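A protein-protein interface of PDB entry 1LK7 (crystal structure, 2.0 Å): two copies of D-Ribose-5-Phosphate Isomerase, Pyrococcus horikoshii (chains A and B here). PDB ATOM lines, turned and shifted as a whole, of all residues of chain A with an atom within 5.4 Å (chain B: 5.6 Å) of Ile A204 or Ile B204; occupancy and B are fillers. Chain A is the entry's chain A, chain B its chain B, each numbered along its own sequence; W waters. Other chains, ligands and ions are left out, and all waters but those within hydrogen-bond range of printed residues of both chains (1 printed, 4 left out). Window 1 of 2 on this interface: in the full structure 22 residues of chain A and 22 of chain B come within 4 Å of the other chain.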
ATOM      1  N   THR A 105       1.764   9.695 -19.943  1.00  0.00           N
ATOM      2  CA  THR A 105       1.654  10.650 -21.008  1.00  0.00           C
ATOM      3  C   THR A 105       0.263  10.638 -21.610  1.00  0.00           C
ATOM      4  O   THR A 105      -0.395  11.678 -21.708  1.00  0.00           O
ATOM      5  CB  THR A 105       2.723  10.331 -22.081  1.00  0.00           C
ATOM      6  OG1 THR A 105       3.996  10.696 -21.578  1.00  0.00           O
ATOM      7  CG2 THR A 105       2.549  11.162 -23.291  1.00  0.00           C
ATOM      8  N   GLU A 139       8.709  10.653 -17.550  1.00  0.00           N
ATOM      9  CA  GLU A 139       9.005  10.045 -18.816  1.00  0.00           C
ATOM     10  C   GLU A 139       9.972  10.969 -19.546  1.00  0.00           C
ATOM     11  O   GLU A 139       9.715  12.172 -19.653  1.00  0.00           O
ATOM     12  CB  GLU A 139       7.738   9.841 -19.630  1.00  0.00           C
ATOM     13  CG  GLU A 139       7.984   9.090 -20.949  1.00  0.00           C
ATOM     14  CD  GLU A 139       6.698   8.668 -21.660  1.00  0.00           C
ATOM     15  OE1 GLU A 139       5.634   8.790 -21.036  1.00  0.00           O
ATOM     16  OE2 GLU A 139       6.769   8.214 -22.832  1.00  0.00           O
ATOM     17  N   VAL A 140      11.100  10.412 -19.978  1.00  0.00           N
ATOM     18  CA  VAL A 140      12.159  11.194 -20.612  1.00  0.00           C
ATOM     19  C   VAL A 140      12.632  10.619 -21.932  1.00  0.00           C
ATOM     20  O   VAL A 140      12.551   9.424 -22.151  1.00  0.00           O
ATOM     21  CB  VAL A 140      13.371  11.346 -19.636  1.00  0.00           C
ATOM     22  CG1 VAL A 140      12.898  11.881 -18.324  1.00  0.00           C
ATOM     23  CG2 VAL A 140      14.062  10.037 -19.362  1.00  0.00           C
ATOM     24  N   ILE A 141      13.073  11.494 -22.824  1.00  0.00           N
ATOM     25  CA  ILE A 141      13.741  11.096 -24.060  1.00  0.00           C
ATOM     26  C   ILE A 141      14.982  10.343 -23.642  1.00  0.00           C
ATOM     27  O   ILE A 141      15.742  10.824 -22.810  1.00  0.00           O
ATOM     28  CB  ILE A 141      14.166  12.335 -24.841  1.00  0.00           C
ATOM     29  CG1 ILE A 141      12.934  12.997 -25.454  1.00  0.00           C
ATOM     30  CG2 ILE A 141      15.215  11.976 -25.879  1.00  0.00           C
ATOM     31  CD1 ILE A 141      12.373  12.310 -26.630  1.00  0.00           C
ATOM     32  N   ASN A 177       9.984   5.706 -24.800  1.00  0.00           N
ATOM     33  CA  ASN A 177      10.808   6.485 -23.890  1.00  0.00           C
ATOM     34  C   ASN A 177      11.216   5.761 -22.606  1.00  0.00           C
ATOM     35  O   ASN A 177      10.728   4.680 -22.300  1.00  0.00           O
ATOM     36  CB  ASN A 177      10.100   7.807 -23.539  1.00  0.00           C
ATOM     37  CG  ASN A 177       9.744   8.618 -24.755  1.00  0.00           C
ATOM     38  OD1 ASN A 177      10.588   8.883 -25.625  1.00  0.00           O
ATOM     39  ND2 ASN A 177       8.478   9.013 -24.842  1.00  0.00           N
ATOM     40  N   ASN A 198       8.241  19.763 -16.405  1.00  0.00           N
ATOM     41  CA  ASN A 198       7.950  19.841 -17.821  1.00  0.00           C
ATOM     42  C   ASN A 198       8.736  20.905 -18.604  1.00  0.00           C
ATOM     43  O   ASN A 198       8.800  20.826 -19.810  1.00  0.00           O
ATOM     44  CB  ASN A 198       6.437  20.003 -18.062  1.00  0.00           C
ATOM     45  CG  ASN A 198       5.678  18.680 -17.928  1.00  0.00           C
ATOM     46  OD1 ASN A 198       4.444  18.655 -17.850  1.00  0.00           O
ATOM     47  ND2 ASN A 198       6.412  17.589 -17.842  1.00  0.00           N
ATOM     48  N   GLY A 202      13.973  17.423 -22.650  1.00  0.00           N
ATOM     49  CA  GLY A 202      14.109  15.985 -22.453  1.00  0.00           C
ATOM     50  C   GLY A 202      12.968  15.405 -21.619  1.00  0.00           C
ATOM     51  O   GLY A 202      12.668  14.227 -21.736  1.00  0.00           O
ATOM     52  N   VAL A 203      12.318  16.211 -20.778  1.00  0.00           N
ATOM     53  CA  VAL A 203      11.214  15.675 -19.963  1.00  0.00           C
ATOM     54  C   VAL A 203       9.958  15.679 -20.827  1.00  0.00           C
ATOM     55  O   VAL A 203       9.555  16.713 -21.291  1.00  0.00           O
ATOM     56  CB  VAL A 203      10.956  16.474 -18.666  1.00  0.00           C
ATOM     57  CG1 VAL A 203       9.543  16.213 -18.147  1.00  0.00           C
ATOM     58  CG2 VAL A 203      11.943  16.120 -17.606  1.00  0.00           C
ATOM     59  N   ILE A 204       9.355  14.509 -21.026  1.00  0.00           N
ATOM     60  CA  ILE A 204       8.177  14.355 -21.845  1.00  0.00           C
ATOM     61  C   ILE A 204       6.916  14.709 -21.046  1.00  0.00           C
ATOM     62  O   ILE A 204       6.070  15.429 -21.522  1.00  0.00           O
ATOM     63  CB  ILE A 204       8.082  12.899 -22.362  1.00  0.00           C
ATOM     64  CG1 ILE A 204       9.301  12.540 -23.244  1.00  0.00           C
ATOM     65  CG2 ILE A 204       6.839  12.674 -23.127  1.00  0.00           C
ATOM     66  CD1 ILE A 204       9.236  13.135 -24.631  1.00  0.00           C
ATOM     67  N   GLU A 205       6.826  14.157 -19.846  1.00  0.00           N
ATOM     68  CA  GLU A 205       5.688  14.320 -18.960  1.00  0.00           C
ATOM     69  C   GLU A 205       6.148  13.845 -17.639  1.00  0.00           C
ATOM     70  O   GLU A 205       7.121  13.072 -17.571  1.00  0.00           O
ATOM     71  CB  GLU A 205       4.501  13.454 -19.405  1.00  0.00           C
ATOM     72  CG  GLU A 205       3.209  13.789 -18.669  1.00  0.00           C
ATOM     73  CD  GLU A 205       2.933  15.283 -18.710  1.00  0.00           C
ATOM     74  OE1 GLU A 205       2.444  15.775 -19.769  1.00  0.00           O
ATOM     75  OE2 GLU A 205       3.248  15.989 -17.704  1.00  0.00           O
ATOM     76  N   ASN A 206       5.462  14.288 -16.590  1.00  0.00           N
ATOM     77  CA  ASN A 206       5.762  13.872 -15.232  1.00  0.00           C
ATOM     78  C   ASN A 206       4.471  13.466 -14.545  1.00  0.00           C
ATOM     79  O   ASN A 206       3.403  13.937 -14.921  1.00  0.00           O
ATOM     80  CB  ASN A 206       6.523  14.970 -14.443  1.00  0.00           C
ATOM     81  CG  ASN A 206       5.704  16.231 -14.219  1.00  0.00           C
ATOM     82  OD1 ASN A 206       5.675  17.147 -15.053  1.00  0.00           O
ATOM     83  ND2 ASN A 206       5.030  16.281 -13.105  1.00  0.00           N
ATOM     84  N   THR B 105      13.451  18.836 -30.664  1.00  0.00           N
ATOM     85  CA  THR B 105      13.579  18.187 -29.372  1.00  0.00           C
ATOM     86  C   THR B 105      15.036  17.926 -28.962  1.00  0.00           C
ATOM     87  O   THR B 105      15.476  18.330 -27.872  1.00  0.00           O
ATOM     88  CB  THR B 105      12.734  16.906 -29.302  1.00  0.00           C
ATOM     89  OG1 THR B 105      11.360  17.271 -29.249  1.00  0.00           O
ATOM     90  CG2 THR B 105      12.945  16.159 -28.015  1.00  0.00           C
ATOM     91  N   GLU B 139       6.299  20.005 -31.661  1.00  0.00           N
ATOM     92  CA  GLU B 139       6.317  18.563 -31.793  1.00  0.00           C
ATOM     93  C   GLU B 139       5.293  17.991 -30.819  1.00  0.00           C
ATOM     94  O   GLU B 139       5.339  18.311 -29.618  1.00  0.00           O
ATOM     95  CB  GLU B 139       7.712  17.995 -31.511  1.00  0.00           C
ATOM     96  CG  GLU B 139       7.799  16.481 -31.444  1.00  0.00           C
ATOM     97  CD  GLU B 139       9.216  15.956 -31.688  1.00  0.00           C
ATOM     98  OE1 GLU B 139      10.142  16.793 -31.643  1.00  0.00           O
ATOM     99  OE2 GLU B 139       9.413  14.705 -31.874  1.00  0.00           O
ATOM    100  N   VAL B 140       4.393  17.150 -31.331  1.00  0.00           N
ATOM    101  CA  VAL B 140       3.288  16.609 -30.508  1.00  0.00           C
ATOM    102  C   VAL B 140       3.115  15.118 -30.558  1.00  0.00           C
ATOM    103  O   VAL B 140       3.455  14.495 -31.549  1.00  0.00           O
ATOM    104  CB  VAL B 140       1.933  17.273 -30.905  1.00  0.00           C
ATOM    105  CG1 VAL B 140       2.049  18.746 -30.792  1.00  0.00           C
ATOM    106  CG2 VAL B 140       1.525  16.930 -32.339  1.00  0.00           C
ATOM    107  N   ILE B 141       2.575  14.543 -29.474  1.00  0.00           N
ATOM    108  CA  ILE B 141       2.245  13.133 -29.419  1.00  0.00           C
ATOM    109  C   ILE B 141       1.130  13.003 -30.433  1.00  0.00           C
ATOM    110  O   ILE B 141       0.186  13.798 -30.408  1.00  0.00           O
ATOM    111  CB  ILE B 141       1.771  12.701 -27.983  1.00  0.00           C
ATOM    112  CG1 ILE B 141       2.904  12.749 -26.978  1.00  0.00           C
ATOM    113  CG2 ILE B 141       1.242  11.306 -28.016  1.00  0.00           C
ATOM    114  CD1 ILE B 141       4.080  11.772 -27.315  1.00  0.00           C
ATOM    115  N   ASN B 177       7.003  11.324 -33.635  1.00  0.00           N
ATOM    116  CA  ASN B 177       5.941  12.256 -33.387  1.00  0.00           C
ATOM    117  C   ASN B 177       5.484  13.092 -34.619  1.00  0.00           C
ATOM    118  O   ASN B 177       6.062  13.012 -35.716  1.00  0.00           O
ATOM    119  CB  ASN B 177       6.370  13.157 -32.207  1.00  0.00           C
ATOM    120  CG  ASN B 177       6.672  12.355 -30.912  1.00  0.00           C
ATOM    121  OD1 ASN B 177       5.924  11.462 -30.525  1.00  0.00           O
ATOM    122  ND2 ASN B 177       7.765  12.699 -30.241  1.00  0.00           N
ATOM    123  N   ASN B 198       4.869  24.167 -23.752  1.00  0.00           N
ATOM    124  CA  ASN B 198       5.330  22.918 -23.145  1.00  0.00           C
ATOM    125  C   ASN B 198       4.473  22.363 -21.984  1.00  0.00           C
ATOM    126  O   ASN B 198       4.508  21.160 -21.732  1.00  0.00           O
ATOM    127  CB  ASN B 198       6.790  23.011 -22.722  1.00  0.00           C
ATOM    128  CG  ASN B 198       7.758  22.883 -23.891  1.00  0.00           C
ATOM    129  OD1 ASN B 198       8.967  23.056 -23.717  1.00  0.00           O
ATOM    130  ND2 ASN B 198       7.248  22.582 -25.070  1.00  0.00           N
ATOM    131  N   ILE B 200       1.227  22.157 -21.984  1.00  0.00           N
ATOM    132  CA  ILE B 200       0.069  21.454 -22.549  1.00  0.00           C
ATOM    133  C   ILE B 200       0.382  19.967 -22.722  1.00  0.00           C
ATOM    134  O   ILE B 200       1.383  19.611 -23.355  1.00  0.00           O
ATOM    135  CB  ILE B 200      -0.270  22.030 -23.925  1.00  0.00           C
ATOM    136  CG1 ILE B 200      -0.618  23.520 -23.815  1.00  0.00           C
ATOM    137  CG2 ILE B 200      -1.375  21.206 -24.593  1.00  0.00           C
ATOM    138  CD1 ILE B 200      -0.762  24.173 -25.156  1.00  0.00           C
ATOM    139  N   GLY B 202       0.730  16.581 -24.236  1.00  0.00           N
ATOM    140  CA  GLY B 202       0.771  16.170 -25.616  1.00  0.00           C
ATOM    141  C   GLY B 202       1.781  17.024 -26.361  1.00  0.00           C
ATOM    142  O   GLY B 202       2.261  16.614 -27.404  1.00  0.00           O
ATOM    143  N   VAL B 203       2.052  18.238 -25.887  1.00  0.00           N
ATOM    144  CA  VAL B 203       3.152  18.991 -26.472  1.00  0.00           C
ATOM    145  C   VAL B 203       4.438  18.502 -25.819  1.00  0.00           C
ATOM    146  O   VAL B 203       4.581  18.513 -24.603  1.00  0.00           O
ATOM    147  CB  VAL B 203       3.024  20.537 -26.317  1.00  0.00           C
ATOM    148  CG1 VAL B 203       4.292  21.227 -26.778  1.00  0.00           C
ATOM    149  CG2 VAL B 203       1.880  21.058 -27.112  1.00  0.00           C
ATOM    150  N   ILE B 204       5.351  18.043 -26.662  1.00  0.00           N
ATOM    151  CA  ILE B 204       6.643  17.540 -26.238  1.00  0.00           C
ATOM    152  C   ILE B 204       7.730  18.621 -26.237  1.00  0.00           C
ATOM    153  O   ILE B 204       8.626  18.604 -25.413  1.00  0.00           O
ATOM    154  CB  ILE B 204       7.027  16.396 -27.230  1.00  0.00           C
ATOM    155  CG1 ILE B 204       6.057  15.217 -27.082  1.00  0.00           C
ATOM    156  CG2 ILE B 204       8.433  15.941 -27.088  1.00  0.00           C
ATOM    157  CD1 ILE B 204       6.112  14.566 -25.732  1.00  0.00           C
ATOM    158  N   GLU B 205       7.740  19.452 -27.257  1.00  0.00           N
ATOM    159  CA  GLU B 205       8.702  20.546 -27.303  1.00  0.00           C
ATOM    160  C   GLU B 205       8.163  21.532 -28.287  1.00  0.00           C
ATOM    161  O   GLU B 205       7.316  21.151 -29.119  1.00  0.00           O
ATOM    162  CB  GLU B 205      10.088  20.039 -27.753  1.00  0.00           C
ATOM    163  CG  GLU B 205      11.172  21.080 -27.660  1.00  0.00           C
ATOM    164  CD  GLU B 205      11.209  21.724 -26.286  1.00  0.00           C
ATOM    165  OE1 GLU B 205      11.796  21.098 -25.394  1.00  0.00           O
ATOM    166  OE2 GLU B 205      10.610  22.818 -26.091  1.00  0.00           O
ATOM    167  N   ASN B 206       8.580  22.796 -28.169  1.00  0.00           N
ATOM    168  CA  ASN B 206       8.262  23.812 -29.167  1.00  0.00           C
ATOM    169  C   ASN B 206       9.511  24.578 -29.669  1.00  0.00           C
ATOM    170  O   ASN B 206      10.525  24.652 -29.006  1.00  0.00           O
ATOM    171  CB  ASN B 206       7.189  24.798 -28.685  1.00  0.00           C
ATOM    172  CG  ASN B 206       7.621  25.614 -27.494  1.00  0.00           C
ATOM    173  OD1 ASN B 206       7.461  25.202 -26.331  1.00  0.00           O
ATOM    174  ND2 ASN B 206       8.193  26.734 -27.757  1.00  0.00           N
HETATM  175  O   HOH W   1       1.053  14.493 -21.519  1.00  0.00           O
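The backbone NH of Ile A204 lies within hydrogen-bond range of the backbone carbonyl oxygen of Glu A139 (2.7 Å). The backbone carbonyl oxygen (O) of Glu B139 sits at hydrogen-bond distance from the backbone NH (N) of Ile B204 (3.0 Å).
Among the printed residues, merely in contact across the chains: Ile A204 with Ile B204 (3.3 Å).
Ile A204 touches one residue of chain B. Of chain A, only Ile A204 (3.3 Å) comes within 4 Å of Ile B204. Glu A139 touches none of the printed residues of chain B. The nearest residue of chain B that does not touch Ile A204 is Val B203 (4.6 Å). The nearest residue of chain A that does not touch Ile B204 is Val A203 (4.6 Å).
Of the 11 printed residues of chain A, 1 touches a printed residue of chain B. Printed residues of chain A that touch a printed residue of chain B: Ile A204. Hydrophobic or aromatic side chains of chain B within 4 Å of the printed part of chain A: Ile B204. Among the printed residues, 1 pair touches across the chains. Among the printed residues, no Asp or Glu carboxylate lies within 4 Å of a Lys or Arg side-chain nitrogen of the other chain.
Ile A204 touches its own counterpart, Ile B204.
Water W1 lies within hydrogen-bond range of the side-chain carboxylate of Glu A205, the backbone carbonyl oxygen of Thr A105 and the backbone NH of Gly B202.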
